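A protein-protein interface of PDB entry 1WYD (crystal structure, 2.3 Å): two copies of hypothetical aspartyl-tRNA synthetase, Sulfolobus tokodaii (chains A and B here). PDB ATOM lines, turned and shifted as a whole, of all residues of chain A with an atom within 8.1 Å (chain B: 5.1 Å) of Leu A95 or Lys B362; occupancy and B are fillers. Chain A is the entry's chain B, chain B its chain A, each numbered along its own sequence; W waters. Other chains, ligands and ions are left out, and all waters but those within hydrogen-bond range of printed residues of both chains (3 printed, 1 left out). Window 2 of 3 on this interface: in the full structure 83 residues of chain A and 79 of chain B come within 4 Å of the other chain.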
ATOM      1  N   TYR A   2      15.350  14.503  30.237  1.00  0.00           N
ATOM      2  CA  TYR A   2      14.668  15.596  29.540  1.00  0.00           C
ATOM      3  C   TYR A   2      13.182  15.637  29.859  1.00  0.00           C
ATOM      4  O   TYR A   2      12.429  16.444  29.317  1.00  0.00           O
ATOM      5  CB  TYR A   2      14.896  15.530  28.008  1.00  0.00           C
ATOM      6  CG  TYR A   2      16.263  15.969  27.535  1.00  0.00           C
ATOM      7  CD1 TYR A   2      16.484  17.265  27.082  1.00  0.00           C
ATOM      8  CD2 TYR A   2      17.339  15.083  27.537  1.00  0.00           C
ATOM      9  CE1 TYR A   2      17.750  17.665  26.617  1.00  0.00           C
ATOM     10  CE2 TYR A   2      18.598  15.465  27.089  1.00  0.00           C
ATOM     11  CZ  TYR A   2      18.802  16.753  26.622  1.00  0.00           C
ATOM     12  OH  TYR A   2      20.061  17.129  26.185  1.00  0.00           O
ATOM     13  N   ARG A   3      12.774  14.748  30.740  1.00  0.00           N
ATOM     14  CA  ARG A   3      11.383  14.579  31.082  1.00  0.00           C
ATOM     15  C   ARG A   3      11.325  14.102  32.510  1.00  0.00           C
ATOM     16  O   ARG A   3      12.328  13.642  33.031  1.00  0.00           O
ATOM     17  CB  ARG A   3      10.750  13.515  30.192  1.00  0.00           C
ATOM     18  CG  ARG A   3      11.642  12.327  29.946  1.00  0.00           C
ATOM     19  CD  ARG A   3      10.906  11.171  29.474  1.00  0.00           C
ATOM     20  NE  ARG A   3      10.552  11.258  28.050  1.00  0.00           N
ATOM     21  CZ  ARG A   3      11.161  10.573  27.081  1.00  0.00           C
ATOM     22  NH1 ARG A   3      12.198   9.791  27.366  1.00  0.00           N
ATOM     23  NH2 ARG A   3      10.734  10.656  25.841  1.00  0.00           N
ATOM     24  N   TRP A  21       6.954  16.200  29.784  1.00  0.00           N
ATOM     25  CA  TRP A  21       7.033  15.262  28.674  1.00  0.00           C
ATOM     26  C   TRP A  21       8.161  15.656  27.744  1.00  0.00           C
ATOM     27  O   TRP A  21       8.492  16.859  27.639  1.00  0.00           O
ATOM     28  CB  TRP A  21       5.736  15.248  27.888  1.00  0.00           C
ATOM     29  CG  TRP A  21       4.684  14.417  28.509  1.00  0.00           C
ATOM     30  CD1 TRP A  21       4.820  13.605  29.582  1.00  0.00           C
ATOM     31  CD2 TRP A  21       3.315  14.310  28.094  1.00  0.00           C
ATOM     32  NE1 TRP A  21       3.628  12.983  29.862  1.00  0.00           N
ATOM     33  CE2 TRP A  21       2.681  13.412  28.974  1.00  0.00           C
ATOM     34  CE3 TRP A  21       2.554  14.892  27.065  1.00  0.00           C
ATOM     35  CZ2 TRP A  21       1.335  13.081  28.869  1.00  0.00           C
ATOM     36  CZ3 TRP A  21       1.223  14.563  26.955  1.00  0.00           C
ATOM     37  CH2 TRP A  21       0.618  13.663  27.849  1.00  0.00           C
ATOM     38  N   ALA A  22       8.762  14.658  27.083  1.00  0.00           N
ATOM     39  CA  ALA A  22       9.657  14.934  25.944  1.00  0.00           C
ATOM     40  C   ALA A  22       9.346  14.021  24.763  1.00  0.00           C
ATOM     41  O   ALA A  22       8.885  12.878  24.939  1.00  0.00           O
ATOM     42  CB  ALA A  22      11.133  14.835  26.336  1.00  0.00           C
ATOM     43  N   GLY A  23       9.582  14.525  23.561  1.00  0.00           N
ATOM     44  CA  GLY A  23       9.345  13.701  22.401  1.00  0.00           C
ATOM     45  C   GLY A  23       9.171  14.443  21.108  1.00  0.00           C
ATOM     46  O   GLY A  23       9.656  15.552  20.952  1.00  0.00           O
ATOM     47  N   TRP A  24       8.462  13.792  20.191  1.00  0.00           N
ATOM     48  CA  TRP A  24       8.280  14.240  18.824  1.00  0.00           C
ATOM     49  C   TRP A  24       6.897  14.836  18.594  1.00  0.00           C
ATOM     50  O   TRP A  24       5.873  14.300  19.029  1.00  0.00           O
ATOM     51  CB  TRP A  24       8.505  13.061  17.864  1.00  0.00           C
ATOM     52  CG  TRP A  24       9.939  12.655  17.705  1.00  0.00           C
ATOM     53  CD1 TRP A  24      10.856  13.174  16.812  1.00  0.00           C
ATOM     54  CD2 TRP A  24      10.644  11.685  18.473  1.00  0.00           C
ATOM     55  NE1 TRP A  24      12.081  12.567  16.976  1.00  0.00           N
ATOM     56  CE2 TRP A  24      11.991  11.655  17.990  1.00  0.00           C
ATOM     57  CE3 TRP A  24      10.285  10.809  19.507  1.00  0.00           C
ATOM     58  CZ2 TRP A  24      12.948  10.776  18.489  1.00  0.00           C
ATOM     59  CZ3 TRP A  24      11.260   9.944  20.021  1.00  0.00           C
ATOM     60  CH2 TRP A  24      12.565   9.931  19.508  1.00  0.00           C
ATOM     61  N   ILE A  59       6.252  29.931  20.843  1.00  0.00           N
ATOM     62  CA  ILE A  59       7.124  28.931  20.258  1.00  0.00           C
ATOM     63  C   ILE A  59       6.306  27.826  19.574  1.00  0.00           C
ATOM     64  O   ILE A  59       6.651  27.400  18.486  1.00  0.00           O
ATOM     65  CB  ILE A  59       8.222  28.421  21.274  1.00  0.00           C
ATOM     66  CG1 ILE A  59       9.392  27.748  20.528  1.00  0.00           C
ATOM     67  CG2 ILE A  59       7.618  27.547  22.409  1.00  0.00           C
ATOM     68  CD1 ILE A  59      10.615  27.508  21.390  1.00  0.00           C
ATOM     69  N   LEU A  63       6.665  25.376  15.540  1.00  0.00           N
ATOM     70  CA  LEU A  63       6.842  23.931  15.582  1.00  0.00           C
ATOM     71  C   LEU A  63       6.369  23.221  14.314  1.00  0.00           C
ATOM     72  O   LEU A  63       5.399  23.625  13.664  1.00  0.00           O
ATOM     73  CB  LEU A  63       6.081  23.363  16.790  1.00  0.00           C
ATOM     74  CG  LEU A  63       6.564  23.694  18.196  1.00  0.00           C
ATOM     75  CD1 LEU A  63       5.728  22.920  19.220  1.00  0.00           C
ATOM     76  CD2 LEU A  63       8.052  23.389  18.377  1.00  0.00           C
ATOM     77  N   SER A  67       9.854  17.537  14.779  1.00  0.00           N
ATOM     78  CA  SER A  67      10.709  18.241  15.736  1.00  0.00           C
ATOM     79  C   SER A  67      10.653  17.607  17.114  1.00  0.00           C
ATOM     80  O   SER A  67       9.620  17.036  17.546  1.00  0.00           O
ATOM     81  CB  SER A  67      10.289  19.685  15.870  1.00  0.00           C
ATOM     82  OG  SER A  67      10.273  20.298  14.603  1.00  0.00           O
ATOM     83  N   VAL A  68      11.767  17.701  17.813  1.00  0.00           N
ATOM     84  CA  VAL A  68      11.877  17.096  19.119  1.00  0.00           C
ATOM     85  C   VAL A  68      11.699  18.188  20.153  1.00  0.00           C
ATOM     86  O   VAL A  68      12.420  19.199  20.129  1.00  0.00           O
ATOM     87  CB  VAL A  68      13.243  16.404  19.276  1.00  0.00           C
ATOM     88  CG1 VAL A  68      13.437  15.913  20.671  1.00  0.00           C
ATOM     89  CG2 VAL A  68      13.412  15.283  18.224  1.00  0.00           C
ATOM     90  N   ILE A  69      10.722  18.002  21.048  1.00  0.00           N
ATOM     91  CA  ILE A  69      10.470  19.010  22.056  1.00  0.00           C
ATOM     92  C   ILE A  69      10.446  18.473  23.483  1.00  0.00           C
ATOM     93  O   ILE A  69      10.264  17.275  23.723  1.00  0.00           O
ATOM     94  CB  ILE A  69       9.161  19.884  21.752  1.00  0.00           C
ATOM     95  CG1 ILE A  69       7.849  19.097  21.945  1.00  0.00           C
ATOM     96  CG2 ILE A  69       9.217  20.528  20.418  1.00  0.00           C
ATOM     97  CD1 ILE A  69       6.610  19.968  21.821  1.00  0.00           C
ATOM     98  N   GLN A  70      10.660  19.401  24.410  1.00  0.00           N
ATOM     99  CA  GLN A  70      10.414  19.233  25.832  1.00  0.00           C
ATOM    100  C   GLN A  70       9.167  20.042  26.131  1.00  0.00           C
ATOM    101  O   GLN A  70       9.056  21.200  25.716  1.00  0.00           O
ATOM    102  CB  GLN A  70      11.567  19.863  26.591  1.00  0.00           C
ATOM    103  CG  GLN A  70      12.117  19.056  27.720  1.00  0.00           C
ATOM    104  CD  GLN A  70      13.321  19.731  28.364  1.00  0.00           C
ATOM    105  OE1 GLN A  70      13.657  19.449  29.515  1.00  0.00           O
ATOM    106  NE2 GLN A  70      13.968  20.617  27.623  1.00  0.00           N
ATOM    107  N   VAL A  71       8.217  19.441  26.838  1.00  0.00           N
ATOM    108  CA  VAL A  71       7.049  20.200  27.300  1.00  0.00           C
ATOM    109  C   VAL A  71       6.729  20.018  28.796  1.00  0.00           C
ATOM    110  O   VAL A  71       6.481  18.917  29.274  1.00  0.00           O
ATOM    111  CB  VAL A  71       5.797  20.013  26.360  1.00  0.00           C
ATOM    112  CG1 VAL A  71       5.432  18.543  26.178  1.00  0.00           C
ATOM    113  CG2 VAL A  71       4.614  20.789  26.874  1.00  0.00           C
ATOM    114  N   ILE A  92       7.651  25.130  26.482  1.00  0.00           N
ATOM    115  CA  ILE A  92       8.108  24.215  25.461  1.00  0.00           C
ATOM    116  C   ILE A  92       9.515  24.615  25.009  1.00  0.00           C
ATOM    117  O   ILE A  92       9.784  25.780  24.674  1.00  0.00           O
ATOM    118  CB  ILE A  92       7.105  24.166  24.250  1.00  0.00           C
ATOM    119  CG1 ILE A  92       5.804  23.423  24.629  1.00  0.00           C
ATOM    120  CG2 ILE A  92       7.765  23.561  22.968  1.00  0.00           C
ATOM    121  CD1 ILE A  92       4.542  23.970  23.948  1.00  0.00           C
ATOM    122  N   THR A  93      10.415  23.646  25.022  1.00  0.00           N
ATOM    123  CA  THR A  93      11.756  23.854  24.522  1.00  0.00           C
ATOM    124  C   THR A  93      11.972  23.062  23.236  1.00  0.00           C
ATOM    125  O   THR A  93      11.583  21.891  23.138  1.00  0.00           O
ATOM    126  CB  THR A  93      12.765  23.441  25.587  1.00  0.00           C
ATOM    127  OG1 THR A  93      12.353  23.993  26.843  1.00  0.00           O
ATOM    128  CG2 THR A  93      14.135  24.092  25.307  1.00  0.00           C
ATOM    129  N   LEU A  94      12.563  23.727  22.250  1.00  0.00           N
ATOM    130  CA  LEU A  94      12.909  23.127  20.971  1.00  0.00           C
ATOM    131  C   LEU A  94      14.285  22.471  21.097  1.00  0.00           C
ATOM    132  O   LEU A  94      15.302  23.160  21.277  1.00  0.00           O
ATOM    133  CB  LEU A  94      12.947  24.206  19.900  1.00  0.00           C
ATOM    134  CG  LEU A  94      12.390  24.028  18.488  1.00  0.00           C
ATOM    135  CD1 LEU A  94      13.076  25.050  17.597  1.00  0.00           C
ATOM    136  CD2 LEU A  94      12.598  22.623  17.954  1.00  0.00           C
ATOM    137  N   LEU A  95      14.326  21.144  21.029  1.00  0.00           N
ATOM    138  CA  LEU A  95      15.593  20.443  21.220  1.00  0.00           C
ATOM    139  C   LEU A  95      16.261  20.299  19.880  1.00  0.00           C
ATOM    140  O   LEU A  95      17.470  20.473  19.752  1.00  0.00           O
ATOM    141  CB  LEU A  95      15.364  19.080  21.866  1.00  0.00           C
ATOM    142  CG  LEU A  95      14.653  19.088  23.219  1.00  0.00           C
ATOM    143  CD1 LEU A  95      14.543  17.686  23.740  1.00  0.00           C
ATOM    144  CD2 LEU A  95      15.378  19.983  24.240  1.00  0.00           C
ATOM    145  N   SER A  96      15.448  19.989  18.878  1.00  0.00           N
ATOM    146  CA  SER A  96      15.918  19.717  17.540  1.00  0.00           C
ATOM    147  C   SER A  96      14.753  19.976  16.543  1.00  0.00           C
ATOM    148  O   SER A  96      13.714  19.285  16.571  1.00  0.00           O
ATOM    149  CB  SER A  96      16.429  18.267  17.480  1.00  0.00           C
ATOM    150  OG  SER A  96      16.963  17.949  16.212  1.00  0.00           O
ATOM    151  N   LYS A  97      14.941  20.982  15.691  1.00  0.00           N
ATOM    152  CA  LYS A  97      13.917  21.423  14.754  1.00  0.00           C
ATOM    153  C   LYS A  97      14.039  20.586  13.488  1.00  0.00           C
ATOM    154  O   LYS A  97      15.128  20.242  13.091  1.00  0.00           O
ATOM    155  CB  LYS A  97      14.113  22.912  14.461  1.00  0.00           C
ATOM    156  CG  LYS A  97      12.909  23.672  13.875  1.00  0.00           C
ATOM    157  CD  LYS A  97      13.355  24.852  12.945  1.00  0.00           C
ATOM    158  CE  LYS A  97      13.930  26.047  13.744  1.00  0.00           C
ATOM    159  NZ  LYS A  97      13.987  27.328  12.955  1.00  0.00           N
ATOM    160  N   ALA A  98      12.922  20.208  12.890  1.00  0.00           N
ATOM    161  CA  ALA A  98      12.943  19.430  11.654  1.00  0.00           C
ATOM    162  C   ALA A  98      12.598  20.305  10.448  1.00  0.00           C
ATOM    163  O   ALA A  98      11.690  21.121  10.509  1.00  0.00           O
ATOM    164  CB  ALA A  98      11.969  18.271  11.749  1.00  0.00           C
ATOM    165  N   PHE B 232      17.473  11.075  24.646  1.00  0.00           N
ATOM    166  CA  PHE B 232      17.357  11.960  25.824  1.00  0.00           C
ATOM    167  C   PHE B 232      18.313  11.684  26.995  1.00  0.00           C
ATOM    168  O   PHE B 232      17.996  11.958  28.144  1.00  0.00           O
ATOM    169  CB  PHE B 232      15.903  12.100  26.288  1.00  0.00           C
ATOM    170  CG  PHE B 232      14.943  12.228  25.172  1.00  0.00           C
ATOM    171  CD1 PHE B 232      14.359  11.089  24.603  1.00  0.00           C
ATOM    172  CD2 PHE B 232      14.578  13.468  24.717  1.00  0.00           C
ATOM    173  CE1 PHE B 232      13.474  11.202  23.587  1.00  0.00           C
ATOM    174  CE2 PHE B 232      13.671  13.592  23.681  1.00  0.00           C
ATOM    175  CZ  PHE B 232      13.134  12.471  23.108  1.00  0.00           C
ATOM    176  N   ASN B 360      26.228  14.259  18.776  1.00  0.00           N
ATOM    177  CA  ASN B 360      25.652  15.455  18.198  1.00  0.00           C
ATOM    178  C   ASN B 360      24.302  15.054  17.589  1.00  0.00           C
ATOM    179  O   ASN B 360      24.087  13.887  17.287  1.00  0.00           O
ATOM    180  CB  ASN B 360      26.583  16.017  17.134  1.00  0.00           C
ATOM    181  CG  ASN B 360      27.778  16.785  17.720  1.00  0.00           C
ATOM    182  OD1 ASN B 360      28.916  16.598  17.282  1.00  0.00           O
ATOM    183  ND2 ASN B 360      27.522  17.665  18.671  1.00  0.00           N
ATOM    184  N   HIS B 361      23.394  16.006  17.426  1.00  0.00           N
ATOM    185  CA  HIS B 361      22.062  15.724  16.869  1.00  0.00           C
ATOM    186  C   HIS B 361      21.588  16.837  15.932  1.00  0.00           C
ATOM    187  O   HIS B 361      20.452  16.822  15.477  1.00  0.00           O
ATOM    188  CB  HIS B 361      21.059  15.551  18.001  1.00  0.00           C
ATOM    189  CG  HIS B 361      20.919  16.774  18.853  1.00  0.00           C
ATOM    190  ND1 HIS B 361      19.781  17.547  18.855  1.00  0.00           N
ATOM    191  CD2 HIS B 361      21.791  17.379  19.697  1.00  0.00           C
ATOM    192  CE1 HIS B 361      19.955  18.574  19.672  1.00  0.00           C
ATOM    193  NE2 HIS B 361      21.168  18.497  20.194  1.00  0.00           N
ATOM    194  N   LYS B 362      22.454  17.817  15.684  1.00  0.00           N
ATOM    195  CA  LYS B 362      22.178  18.913  14.759  1.00  0.00           C
ATOM    196  C   LYS B 362      23.026  18.721  13.510  1.00  0.00           C
ATOM    197  O   LYS B 362      24.235  18.462  13.608  1.00  0.00           O
ATOM    198  CB  LYS B 362      22.516  20.275  15.395  1.00  0.00           C
ATOM    199  CG  LYS B 362      21.488  20.802  16.453  1.00  0.00           C
ATOM    200  CD  LYS B 362      21.994  22.102  17.158  1.00  0.00           C
ATOM    201  CE  LYS B 362      21.285  22.407  18.496  1.00  0.00           C
ATOM    202  NZ  LYS B 362      19.838  22.770  18.343  1.00  0.00           N
ATOM    203  N   ARG B 363      22.402  18.848  12.339  1.00  0.00           N
ATOM    204  CA  ARG B 363      23.114  18.709  11.063  1.00  0.00           C
ATOM    205  C   ARG B 363      24.294  19.671  10.986  1.00  0.00           C
ATOM    206  O   ARG B 363      25.388  19.252  10.664  1.00  0.00           O
ATOM    207  CB  ARG B 363      22.178  18.942   9.871  1.00  0.00           C
ATOM    208  CG  ARG B 363      22.886  19.248   8.534  1.00  0.00           C
ATOM    209  CD  ARG B 363      22.023  19.018   7.300  1.00  0.00           C
ATOM    210  NE  ARG B 363      22.794  18.248   6.329  1.00  0.00           N
ATOM    211  CZ  ARG B 363      22.304  17.465   5.404  1.00  0.00           C
ATOM    212  NH1 ARG B 363      21.013  17.298   5.269  1.00  0.00           N
ATOM    213  NH2 ARG B 363      23.124  16.832   4.596  1.00  0.00           N
ATOM    214  N   GLU B 364      24.046  20.943  11.292  1.00  0.00           N
ATOM    215  CA  GLU B 364      25.064  22.000  11.243  1.00  0.00           C
ATOM    216  C   GLU B 364      26.355  21.659  11.999  1.00  0.00           C
ATOM    217  O   GLU B 364      27.464  21.801  11.456  1.00  0.00           O
ATOM    218  CB  GLU B 364      24.491  23.338  11.774  1.00  0.00           C
ATOM    219  CG  GLU B 364      24.445  24.482  10.753  1.00  0.00           C
ATOM    220  CD  GLU B 364      23.789  25.754  11.327  1.00  0.00           C
ATOM    221  OE1 GLU B 364      24.530  26.691  11.724  1.00  0.00           O
ATOM    222  OE2 GLU B 364      22.528  25.827  11.386  1.00  0.00           O
ATOM    223  N   VAL B 365      26.209  21.214  13.247  1.00  0.00           N
ATOM    224  CA  VAL B 365      27.374  20.956  14.085  1.00  0.00           C
ATOM    225  C   VAL B 365      28.124  19.698  13.669  1.00  0.00           C
ATOM    226  O   VAL B 365      29.348  19.636  13.800  1.00  0.00           O
ATOM    227  CB  VAL B 365      27.042  20.985  15.583  1.00  0.00           C
ATOM    228  CG1 VAL B 365      26.337  22.310  15.933  1.00  0.00           C
ATOM    229  CG2 VAL B 365      26.197  19.773  16.006  1.00  0.00           C
ATOM    230  N   LEU B 366      27.396  18.724  13.128  1.00  0.00           N
ATOM    231  CA  LEU B 366      28.007  17.526  12.551  1.00  0.00           C
ATOM    232  C   LEU B 366      28.864  17.879  11.322  1.00  0.00           C
ATOM    233  O   LEU B 366      29.938  17.328  11.120  1.00  0.00           O
ATOM    234  CB  LEU B 366      26.921  16.530  12.129  1.00  0.00           C
ATOM    235  CG  LEU B 366      26.609  15.170  12.782  1.00  0.00           C
ATOM    236  CD1 LEU B 366      27.419  14.862  13.998  1.00  0.00           C
ATOM    237  CD2 LEU B 366      25.135  15.058  13.105  1.00  0.00           C
ATOM    238  N   PHE B 387      19.566  13.630  10.199  1.00  0.00           N
ATOM    239  CA  PHE B 387      19.525  14.635  11.229  1.00  0.00           C
ATOM    240  C   PHE B 387      18.719  15.858  10.814  1.00  0.00           C
ATOM    241  O   PHE B 387      18.615  16.821  11.572  1.00  0.00           O
ATOM    242  CB  PHE B 387      20.942  14.979  11.689  1.00  0.00           C
ATOM    243  CG  PHE B 387      21.617  13.845  12.396  1.00  0.00           C
ATOM    244  CD1 PHE B 387      22.149  12.781  11.684  1.00  0.00           C
ATOM    245  CD2 PHE B 387      21.683  13.820  13.782  1.00  0.00           C
ATOM    246  CE1 PHE B 387      22.769  11.724  12.329  1.00  0.00           C
ATOM    247  CE2 PHE B 387      22.296  12.762  14.444  1.00  0.00           C
ATOM    248  CZ  PHE B 387      22.841  11.702  13.716  1.00  0.00           C
ATOM    249  N   PRO B 393      18.463  14.459  21.230  1.00  0.00           N
ATOM    250  CA  PRO B 393      19.646  14.204  22.023  1.00  0.00           C
ATOM    251  C   PRO B 393      19.768  12.727  22.361  1.00  0.00           C
ATOM    252  O   PRO B 393      18.787  12.052  22.727  1.00  0.00           O
ATOM    253  CB  PRO B 393      19.430  15.077  23.275  1.00  0.00           C
ATOM    254  CG  PRO B 393      18.563  16.208  22.789  1.00  0.00           C
ATOM    255  CD  PRO B 393      17.667  15.590  21.728  1.00  0.00           C
HETATM  256  O   HOH W   1      19.558  20.193  22.376  1.00  0.00           O
HETATM  257  O   HOH W   2      17.626  22.331  15.872  1.00  0.00           O
HETATM  258  O   HOH W   3      18.060  16.481  14.026  1.00  0.00           O
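The backbone carbonyl oxygen of Pro B393 lies within hydrogen-bond range of the backbone NH of Phe B232 (2.5 Å).
OE1 of Gln A70 sits close to O of Tyr A2 (3.3 Å).
NH2 of Arg A3 lies within hydrogen-bond range of O of Ala A22 (3.0 Å).
The backbone NH (N) of Leu A95 sits at hydrogen-bond distance from the backbone carbonyl oxygen (O) of Val A68 (2.9 Å).
N of Val A68 is in hydrogen-bond range of O of Ser A96 (2.8 Å).
Among the printed residues, pairs that only touch across the chains: Tyr A2 with Phe B232, Tyr A2 with Pro B393, Arg A3 with Phe B232, Ala A22 with Phe B232, Val A68 with Phe B232, Leu A95 with His B361, Leu A95 with Lys B362 and Ser A96 with His B361.
Printed residues of chain B within 4 Å of Leu A95: His B361 and Lys B362.
Lys B362 touches one residue of chain A.
Of the printed residues of chain A, Phe B232 touches Tyr A2, Arg A3, Ala A22 and Val A68.
Of the printed residues of chain B, Val A68 touches Phe B232.
Of the printed residues of chain A, His B361 touches Leu A95 (3.1 Å) and Ser A96 (3.7 Å).
Of the printed residues of chain B, Ser A96 touches His B361 (3.7 Å).
Gln A70 touches none of the printed residues of chain B.
The nearest printed residue of chain B that does not touch Leu A95 is Pro B393 (4.2 Å).
The nearest printed residue of chain B that does not touch Ser A96 is Lys B362 (5.0 Å).
Printed residues of chain B that touch a printed residue of chain A: Phe B232, His B361, Lys B362 and Pro B393.
Among the printed residues, no Asp or Glu carboxylate lies within 4 Å of a Lys or Arg side-chain nitrogen of the other chain.
No position is printed for both chains.
Of the 8 pairs that touch across the chains among the printed residues, none has its exchanged pair printed and touching as well.
Water W3 lies within hydrogen-bond range of O of Phe B387 (2.5 Å), O of His B361 (2.8 Å) and OG of Ser A96 (2.9 Å).
Water W2 lies within hydrogen-bond range of N of Lys A97 (3.0 Å) and NZ of Lys B362 (3.3 Å).
Water W1 lies within hydrogen-bond range of NE2 of His B361 (3.2 Å) and O of Leu A95 (3.4 Å).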
